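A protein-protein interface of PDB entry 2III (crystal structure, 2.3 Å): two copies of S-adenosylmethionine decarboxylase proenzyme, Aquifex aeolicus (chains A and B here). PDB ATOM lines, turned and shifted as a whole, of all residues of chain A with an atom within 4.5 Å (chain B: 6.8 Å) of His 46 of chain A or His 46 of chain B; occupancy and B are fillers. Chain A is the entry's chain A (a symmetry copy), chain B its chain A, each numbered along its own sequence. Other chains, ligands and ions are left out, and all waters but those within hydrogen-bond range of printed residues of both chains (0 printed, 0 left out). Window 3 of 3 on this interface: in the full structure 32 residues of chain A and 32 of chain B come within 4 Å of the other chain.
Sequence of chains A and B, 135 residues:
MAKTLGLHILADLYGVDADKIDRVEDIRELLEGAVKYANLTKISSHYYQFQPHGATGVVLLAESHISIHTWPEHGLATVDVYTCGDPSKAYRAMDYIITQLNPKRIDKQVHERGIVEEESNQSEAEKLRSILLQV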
ATOM      1  N   SER A  44       5.232 -20.795  17.424  1.00  0.00           N
ATOM      2  CA  SER A  44       4.373 -21.623  16.584  1.00  0.00           C
ATOM      3  C   SER A  44       3.174 -20.815  16.084  1.00  0.00           C
ATOM      4  O   SER A  44       2.947 -19.687  16.517  1.00  0.00           O
ATOM      5  CB  SER A  44       3.872 -22.830  17.378  1.00  0.00           C
ATOM      6  OG  SER A  44       3.073 -22.423  18.477  1.00  0.00           O
ATOM      7  N   SER A  45       2.407 -21.402  15.174  1.00  0.00           N
ATOM      8  CA  SER A  45       1.238 -20.734  14.622  1.00  0.00           C
ATOM      9  C   SER A  45       0.152 -21.765  14.326  1.00  0.00           C
ATOM     10  O   SER A  45       0.436 -22.870  13.855  1.00  0.00           O
ATOM     11  CB  SER A  45       1.612 -19.972  13.345  1.00  0.00           C
ATOM     12  OG  SER A  45       2.005 -20.854  12.308  1.00  0.00           O
ATOM     13  N   HIS A  46      -1.096 -21.399  14.604  1.00  0.00           N
ATOM     14  CA  HIS A  46      -2.213 -22.306  14.393  1.00  0.00           C
ATOM     15  C   HIS A  46      -3.398 -21.622  13.742  1.00  0.00           C
ATOM     16  O   HIS A  46      -3.804 -20.531  14.151  1.00  0.00           O
ATOM     17  CB  HIS A  46      -2.603 -22.925  15.732  1.00  0.00           C
ATOM     18  CG  HIS A  46      -1.420 -23.392  16.518  1.00  0.00           C
ATOM     19  ND1 HIS A  46      -0.733 -22.566  17.381  1.00  0.00           N
ATOM     20  CD2 HIS A  46      -0.717 -24.547  16.461  1.00  0.00           C
ATOM     21  CE1 HIS A  46       0.344 -23.191  17.821  1.00  0.00           C
ATOM     22  NE2 HIS A  46       0.377 -24.394  17.276  1.00  0.00           N
ATOM     23  N   TYR A  47      -3.939 -22.279  12.719  1.00  0.00           N
ATOM     24  CA  TYR A  47      -5.063 -21.752  11.966  1.00  0.00           C
ATOM     25  C   TYR A  47      -6.243 -22.695  11.902  1.00  0.00           C
ATOM     26  O   TYR A  47      -6.099 -23.908  12.050  1.00  0.00           O
ATOM     27  CB  TYR A  47      -4.620 -21.421  10.549  1.00  0.00           C
ATOM     28  CG  TYR A  47      -3.436 -20.495  10.507  1.00  0.00           C
ATOM     29  CD1 TYR A  47      -2.138 -20.977  10.690  1.00  0.00           C
ATOM     30  CD2 TYR A  47      -3.613 -19.125  10.322  1.00  0.00           C
ATOM     31  CE1 TYR A  47      -1.041 -20.112  10.693  1.00  0.00           C
ATOM     32  CE2 TYR A  47      -2.531 -18.252  10.324  1.00  0.00           C
ATOM     33  CZ  TYR A  47      -1.250 -18.749  10.510  1.00  0.00           C
ATOM     34  OH  TYR A  47      -0.186 -17.875  10.516  1.00  0.00           O
ATOM     35  N   THR A  56      -9.669 -18.465  11.869  1.00  0.00           N
ATOM     36  CA  THR A  56      -8.993 -18.015  13.072  1.00  0.00           C
ATOM     37  C   THR A  56      -7.508 -18.282  12.873  1.00  0.00           C
ATOM     38  O   THR A  56      -7.115 -19.255  12.219  1.00  0.00           O
ATOM     39  CB  THR A  56      -9.466 -18.775  14.320  1.00  0.00           C
ATOM     40  OG1 THR A  56     -10.796 -18.361  14.653  1.00  0.00           O
ATOM     41  CG2 THR A  56      -8.545 -18.492  15.498  1.00  0.00           C
ATOM     42  N   GLY A  57      -6.683 -17.398  13.414  1.00  0.00           N
ATOM     43  CA  GLY A  57      -5.249 -17.561  13.301  1.00  0.00           C
ATOM     44  C   GLY A  57      -4.624 -17.037  14.574  1.00  0.00           C
ATOM     45  O   GLY A  57      -4.976 -15.949  15.030  1.00  0.00           O
ATOM     46  N   VAL A  58      -3.729 -17.815  15.171  1.00  0.00           N
ATOM     47  CA  VAL A  58      -3.059 -17.390  16.391  1.00  0.00           C
ATOM     48  C   VAL A  58      -1.581 -17.723  16.293  1.00  0.00           C
ATOM     49  O   VAL A  58      -1.203 -18.797  15.825  1.00  0.00           O
ATOM     50  CB  VAL A  58      -3.640 -18.083  17.636  1.00  0.00           C
ATOM     51  CG1 VAL A  58      -3.399 -19.577  17.553  1.00  0.00           C
ATOM     52  CG2 VAL A  58      -2.998 -17.509  18.900  1.00  0.00           C
ATOM     53  N   LEU A  60       1.908 -17.770  18.649  1.00  0.00           N
ATOM     54  CA  LEU A  60       2.529 -17.623  19.960  1.00  0.00           C
ATOM     55  C   LEU A  60       3.908 -17.026  19.669  1.00  0.00           C
ATOM     56  O   LEU A  60       4.658 -17.560  18.852  1.00  0.00           O
ATOM     57  CB  LEU A  60       2.672 -18.982  20.665  1.00  0.00           C
ATOM     58  CG  LEU A  60       1.410 -19.619  21.270  1.00  0.00           C
ATOM     59  CD1 LEU A  60       0.451 -20.026  20.170  1.00  0.00           C
ATOM     60  CD2 LEU A  60       1.792 -20.832  22.092  1.00  0.00           C
ATOM     61  N   ILE B  27      -0.684 -24.287  33.715  1.00  0.00           N
ATOM     62  CA  ILE B  27      -1.502 -23.549  32.752  1.00  0.00           C
ATOM     63  C   ILE B  27      -2.483 -24.469  32.038  1.00  0.00           C
ATOM     64  O   ILE B  27      -3.660 -24.128  31.873  1.00  0.00           O
ATOM     65  CB  ILE B  27      -0.616 -22.823  31.704  1.00  0.00           C
ATOM     66  CG1 ILE B  27       0.263 -21.793  32.406  1.00  0.00           C
ATOM     67  CG2 ILE B  27      -1.472 -22.147  30.653  1.00  0.00           C
ATOM     68  CD1 ILE B  27      -0.503 -20.852  33.291  1.00  0.00           C
ATOM     69  N   ARG B  28      -1.988 -25.637  31.631  1.00  0.00           N
ATOM     70  CA  ARG B  28      -2.796 -26.631  30.942  1.00  0.00           C
ATOM     71  C   ARG B  28      -3.964 -27.063  31.804  1.00  0.00           C
ATOM     72  O   ARG B  28      -5.105 -27.053  31.350  1.00  0.00           O
ATOM     73  CB  ARG B  28      -1.934 -27.841  30.572  1.00  0.00           C
ATOM     74  CG  ARG B  28      -2.697 -29.078  30.111  1.00  0.00           C
ATOM     75  CD  ARG B  28      -1.776 -29.982  29.294  1.00  0.00           C
ATOM     76  NE  ARG B  28      -1.870 -29.670  27.868  1.00  0.00           N
ATOM     77  CZ  ARG B  28      -0.890 -29.848  26.989  1.00  0.00           C
ATOM     78  NH1 ARG B  28       0.282 -30.331  27.383  1.00  0.00           N
ATOM     79  NH2 ARG B  28      -1.090 -29.554  25.711  1.00  0.00           N
ATOM     80  N   LEU B  31      -6.443 -23.948  32.120  1.00  0.00           N
ATOM     81  CA  LEU B  31      -7.256 -23.673  30.937  1.00  0.00           C
ATOM     82  C   LEU B  31      -8.188 -24.828  30.561  1.00  0.00           C
ATOM     83  O   LEU B  31      -9.286 -24.599  30.042  1.00  0.00           O
ATOM     84  CB  LEU B  31      -6.362 -23.302  29.740  1.00  0.00           C
ATOM     85  CG  LEU B  31      -5.508 -22.028  29.834  1.00  0.00           C
ATOM     86  CD1 LEU B  31      -4.990 -21.667  28.451  1.00  0.00           C
ATOM     87  CD2 LEU B  31      -6.332 -20.878  30.384  1.00  0.00           C
ATOM     88  N   ILE B  43     -11.128 -26.195  19.791  1.00  0.00           N
ATOM     89  CA  ILE B  43     -10.701 -26.645  18.476  1.00  0.00           C
ATOM     90  C   ILE B  43      -9.358 -27.319  18.764  1.00  0.00           C
ATOM     91  O   ILE B  43      -9.147 -28.487  18.440  1.00  0.00           O
ATOM     92  CB  ILE B  43     -10.459 -25.471  17.510  1.00  0.00           C
ATOM     93  CG1 ILE B  43     -11.791 -24.837  17.102  1.00  0.00           C
ATOM     94  CG2 ILE B  43      -9.678 -25.957  16.298  1.00  0.00           C
ATOM     95  CD1 ILE B  43     -11.633 -23.597  16.240  1.00  0.00           C
ATOM     96  N   SER B  44      -8.469 -26.559  19.403  1.00  0.00           N
ATOM     97  CA  SER B  44      -7.135 -27.026  19.762  1.00  0.00           C
ATOM     98  C   SER B  44      -6.550 -26.164  20.881  1.00  0.00           C
ATOM     99  O   SER B  44      -7.113 -25.135  21.250  1.00  0.00           O
ATOM    100  CB  SER B  44      -6.214 -26.965  18.543  1.00  0.00           C
ATOM    101  OG  SER B  44      -6.054 -25.630  18.090  1.00  0.00           O
ATOM    102  N   SER B  45      -5.411 -26.588  21.417  1.00  0.00           N
ATOM    103  CA  SER B  45      -4.757 -25.852  22.489  1.00  0.00           C
ATOM    104  C   SER B  45      -3.243 -25.988  22.352  1.00  0.00           C
ATOM    105  O   SER B  45      -2.728 -27.058  22.017  1.00  0.00           O
ATOM    106  CB  SER B  45      -5.218 -26.377  23.855  1.00  0.00           C
ATOM    107  OG  SER B  45      -4.797 -27.713  24.069  1.00  0.00           O
ATOM    108  N   HIS B  46      -2.531 -24.896  22.615  1.00  0.00           N
ATOM    109  CA  HIS B  46      -1.081 -24.894  22.490  1.00  0.00           C
ATOM    110  C   HIS B  46      -0.403 -24.198  23.653  1.00  0.00           C
ATOM    111  O   HIS B  46      -0.800 -23.101  24.055  1.00  0.00           O
ATOM    112  CB  HIS B  46      -0.703 -24.242  21.163  1.00  0.00           C
ATOM    113  CG  HIS B  46      -1.534 -24.734  20.024  1.00  0.00           C
ATOM    114  ND1 HIS B  46      -2.738 -24.154  19.680  1.00  0.00           N
ATOM    115  CD2 HIS B  46      -1.410 -25.833  19.243  1.00  0.00           C
ATOM    116  CE1 HIS B  46      -3.320 -24.877  18.741  1.00  0.00           C
ATOM    117  NE2 HIS B  46      -2.535 -25.902  18.459  1.00  0.00           N
ATOM    118  N   TYR B  47       0.622 -24.858  24.187  1.00  0.00           N
ATOM    119  CA  TYR B  47       1.365 -24.347  25.325  1.00  0.00           C
ATOM    120  C   TYR B  47       2.853 -24.243  25.078  1.00  0.00           C
ATOM    121  O   TYR B  47       3.407 -24.933  24.224  1.00  0.00           O
ATOM    122  CB  TYR B  47       1.128 -25.240  26.535  1.00  0.00           C
ATOM    123  CG  TYR B  47      -0.331 -25.418  26.854  1.00  0.00           C
ATOM    124  CD1 TYR B  47      -1.115 -26.336  26.151  1.00  0.00           C
ATOM    125  CD2 TYR B  47      -0.942 -24.639  27.836  1.00  0.00           C
ATOM    126  CE1 TYR B  47      -2.479 -26.472  26.419  1.00  0.00           C
ATOM    127  CE2 TYR B  47      -2.299 -24.763  28.111  1.00  0.00           C
ATOM    128  CZ  TYR B  47      -3.062 -25.679  27.402  1.00  0.00           C
ATOM    129  OH  TYR B  47      -4.406 -25.789  27.678  1.00  0.00           O
ATOM    130  N   TYR B  48       3.501 -23.366  25.834  1.00  0.00           N
ATOM    131  CA  TYR B  48       4.936 -23.192  25.714  1.00  0.00           C
ATOM    132  C   TYR B  48       5.563 -22.921  27.076  1.00  0.00           C
ATOM    133  O   TYR B  48       5.073 -22.098  27.842  1.00  0.00           O
ATOM    134  CB  TYR B  48       5.270 -22.045  24.763  1.00  0.00           C
ATOM    135  CG  TYR B  48       6.742 -21.993  24.441  1.00  0.00           C
ATOM    136  CD1 TYR B  48       7.329 -22.957  23.621  1.00  0.00           C
ATOM    137  CD2 TYR B  48       7.563 -21.009  24.994  1.00  0.00           C
ATOM    138  CE1 TYR B  48       8.699 -22.944  23.359  1.00  0.00           C
ATOM    139  CE2 TYR B  48       8.936 -20.986  24.738  1.00  0.00           C
ATOM    140  CZ  TYR B  48       9.495 -21.958  23.921  1.00  0.00           C
ATOM    141  OH  TYR B  48      10.845 -21.944  23.671  1.00  0.00           O
ATOM    142  N   THR B  56       3.119 -19.865  28.304  1.00  0.00           N
ATOM    143  CA  THR B  56       2.069 -19.297  27.478  1.00  0.00           C
ATOM    144  C   THR B  56       1.095 -20.423  27.161  1.00  0.00           C
ATOM    145  O   THR B  56       1.487 -21.587  27.023  1.00  0.00           O
ATOM    146  CB  THR B  56       2.613 -18.732  26.160  1.00  0.00           C
ATOM    147  OG1 THR B  56       3.351 -17.533  26.423  1.00  0.00           O
ATOM    148  CG2 THR B  56       1.472 -18.415  25.203  1.00  0.00           C
ATOM    149  N   GLY B  57      -0.181 -20.078  27.076  1.00  0.00           N
ATOM    150  CA  GLY B  57      -1.193 -21.065  26.763  1.00  0.00           C
ATOM    151  C   GLY B  57      -2.260 -20.383  25.936  1.00  0.00           C
ATOM    152  O   GLY B  57      -2.708 -19.292  26.289  1.00  0.00           O
ATOM    153  N   VAL B  58      -2.644 -20.996  24.823  1.00  0.00           N
ATOM    154  CA  VAL B  58      -3.678 -20.429  23.973  1.00  0.00           C
ATOM    155  C   VAL B  58      -4.630 -21.529  23.538  1.00  0.00           C
ATOM    156  O   VAL B  58      -4.208 -22.635  23.198  1.00  0.00           O
ATOM    157  CB  VAL B  58      -3.088 -19.764  22.716  1.00  0.00           C
ATOM    158  CG1 VAL B  58      -2.398 -20.806  21.858  1.00  0.00           C
ATOM    159  CG2 VAL B  58      -4.196 -19.069  21.923  1.00  0.00           C
ATOM    160  N   VAL B  59      -5.919 -21.228  23.565  1.00  0.00           N
ATOM    161  CA  VAL B  59      -6.928 -22.193  23.159  1.00  0.00           C
ATOM    162  C   VAL B  59      -7.795 -21.561  22.084  1.00  0.00           C
ATOM    163  O   VAL B  59      -8.376 -20.497  22.299  1.00  0.00           O
ATOM    164  CB  VAL B  59      -7.844 -22.580  24.333  1.00  0.00           C
ATOM    165  CG1 VAL B  59      -8.776 -23.724  23.919  1.00  0.00           C
ATOM    166  CG2 VAL B  59      -7.010 -22.959  25.545  1.00  0.00           C
ATOM    167  N   LEU B  60      -7.858 -22.196  20.917  1.00  0.00           N
ATOM    168  CA  LEU B  60      -8.712 -21.706  19.842  1.00  0.00           C
ATOM    169  C   LEU B  60     -10.081 -22.330  20.123  1.00  0.00           C
ATOM    170  O   LEU B  60     -10.190 -23.545  20.292  1.00  0.00           O
ATOM    171  CB  LEU B  60      -8.192 -22.155  18.467  1.00  0.00           C
ATOM    172  CG  LEU B  60      -6.959 -21.438  17.892  1.00  0.00           C
ATOM    173  CD1 LEU B  60      -5.733 -21.759  18.722  1.00  0.00           C
ATOM    174  CD2 LEU B  60      -6.736 -21.873  16.459  1.00  0.00           C
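ND1 of His 46 of chain B sits at hydrogen-bond distance from ND1 of His 46 of chain A, 3.4 Å away.
The backbone NH of Leu 60 of chain B sits at hydrogen-bond distance from the backbone carbonyl oxygen of Ser 44 of chain B (3.1 Å).
N of Leu 60 of chain A is in hydrogen-bond range of O of Ser 44 of chain A, 3.0 Å away.
The backbone carbonyl oxygen (O) of Leu 60 of chain B lies within hydrogen-bond range of the backbone NH (N) of Ile 43 of chain B, at 2.9 Å.
The backbone carbonyl oxygen (O) of Val 58 of chain B sits at hydrogen-bond distance from the backbone NH (N) of His 46 of chain B, 2.9 Å away.
The backbone NH (N) of His 46 of chain A lies within hydrogen-bond range of the backbone carbonyl oxygen (O) of Val 58 of chain A (2.9 Å).
O of Thr 56 of chain B is in hydrogen-bond range of N of Tyr 48 of chain B (2.9 Å).
Among the printed residues, pairs that only touch across the chains: His 46 of chain A with Leu 60 of chain B (3.97 Å), Thr 56 of chain A with Leu 60 of chain B (3.95 Å), Val 58 of chain A with Val 58 of chain B (3.6 Å), Val 58 of chain A with Leu 60 of chain B (3.4 Å), Leu 60 of chain A with His 46 of chain B (3.96 Å), Leu 60 of chain A with Thr 56 of chain B (3.95 Å) and Leu 60 of chain A with Val 58 of chain B (3.4 Å).
His 46 of chain A touches just these residues of chain B: His 46 (3.0 Å) and Leu 60 (3.97 Å).
Printed residues of chain B within 4 Å of Thr 56 of chain A: Leu 60 (3.95 Å).
Of the printed residues of chain B, Val 58 of chain A touches Val 58 (3.6 Å) and Leu 60 (3.4 Å).
Printed residues of chain B within 4 Å of Leu 60 of chain A: His 46 (3.96 Å), Thr 56 (3.95 Å) and Val 58 (3.4 Å).
His 46 of chain B touches just these residues of chain A: His 46 and Leu 60.
Of the printed residues of chain A, Thr 56 of chain B touches Leu 60 (3.95 Å).
Printed residues of chain A within 4 Å of Leu 60 of chain B: His 46, Thr 56 and Val 58.
The nearest residue of chain B that does not touch His 46 of chain A is Ser 44 of chain B (5.0 Å).
The nearest printed residue of chain A that does not touch His 46 of chain B is Ser 44 of chain A (5.0 Å).
Printed residues of chain A that touch a printed residue of chain B: His 46, Thr 56, Val 58 and Leu 60.
Hydrophobic or aromatic side chains of chain A that line the printed part of chain B: His 46, Val 58 and Leu 60.
Of the 14 printed residues of chain B, 4 touch a printed residue of chain A.
Hydrophobic or aromatic side chains of chain B within 4 Å of the printed part of chain A: His 46, Val 58 and Leu 60.
Among the printed residues, no Asp or Glu carboxylate lies within 4 Å of a Lys or Arg side-chain nitrogen of the other chain.
His 46 of chain B touches its own counterpart, His 46 of chain A.
His 46 of chain A touches Leu 60 of chain B, and with the chains exchanged Leu 60 of chain A touches His 46 of chain B.
Thr 56 of chain A touches Leu 60 of chain B, and with the chains exchanged Leu 60 of chain A touches Thr 56 of chain B.
Val 58 of chain A touches Leu 60 of chain B, and with the chains exchanged Leu 60 of chain A touches Val 58 of chain B.
8 positions are printed for both chains.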
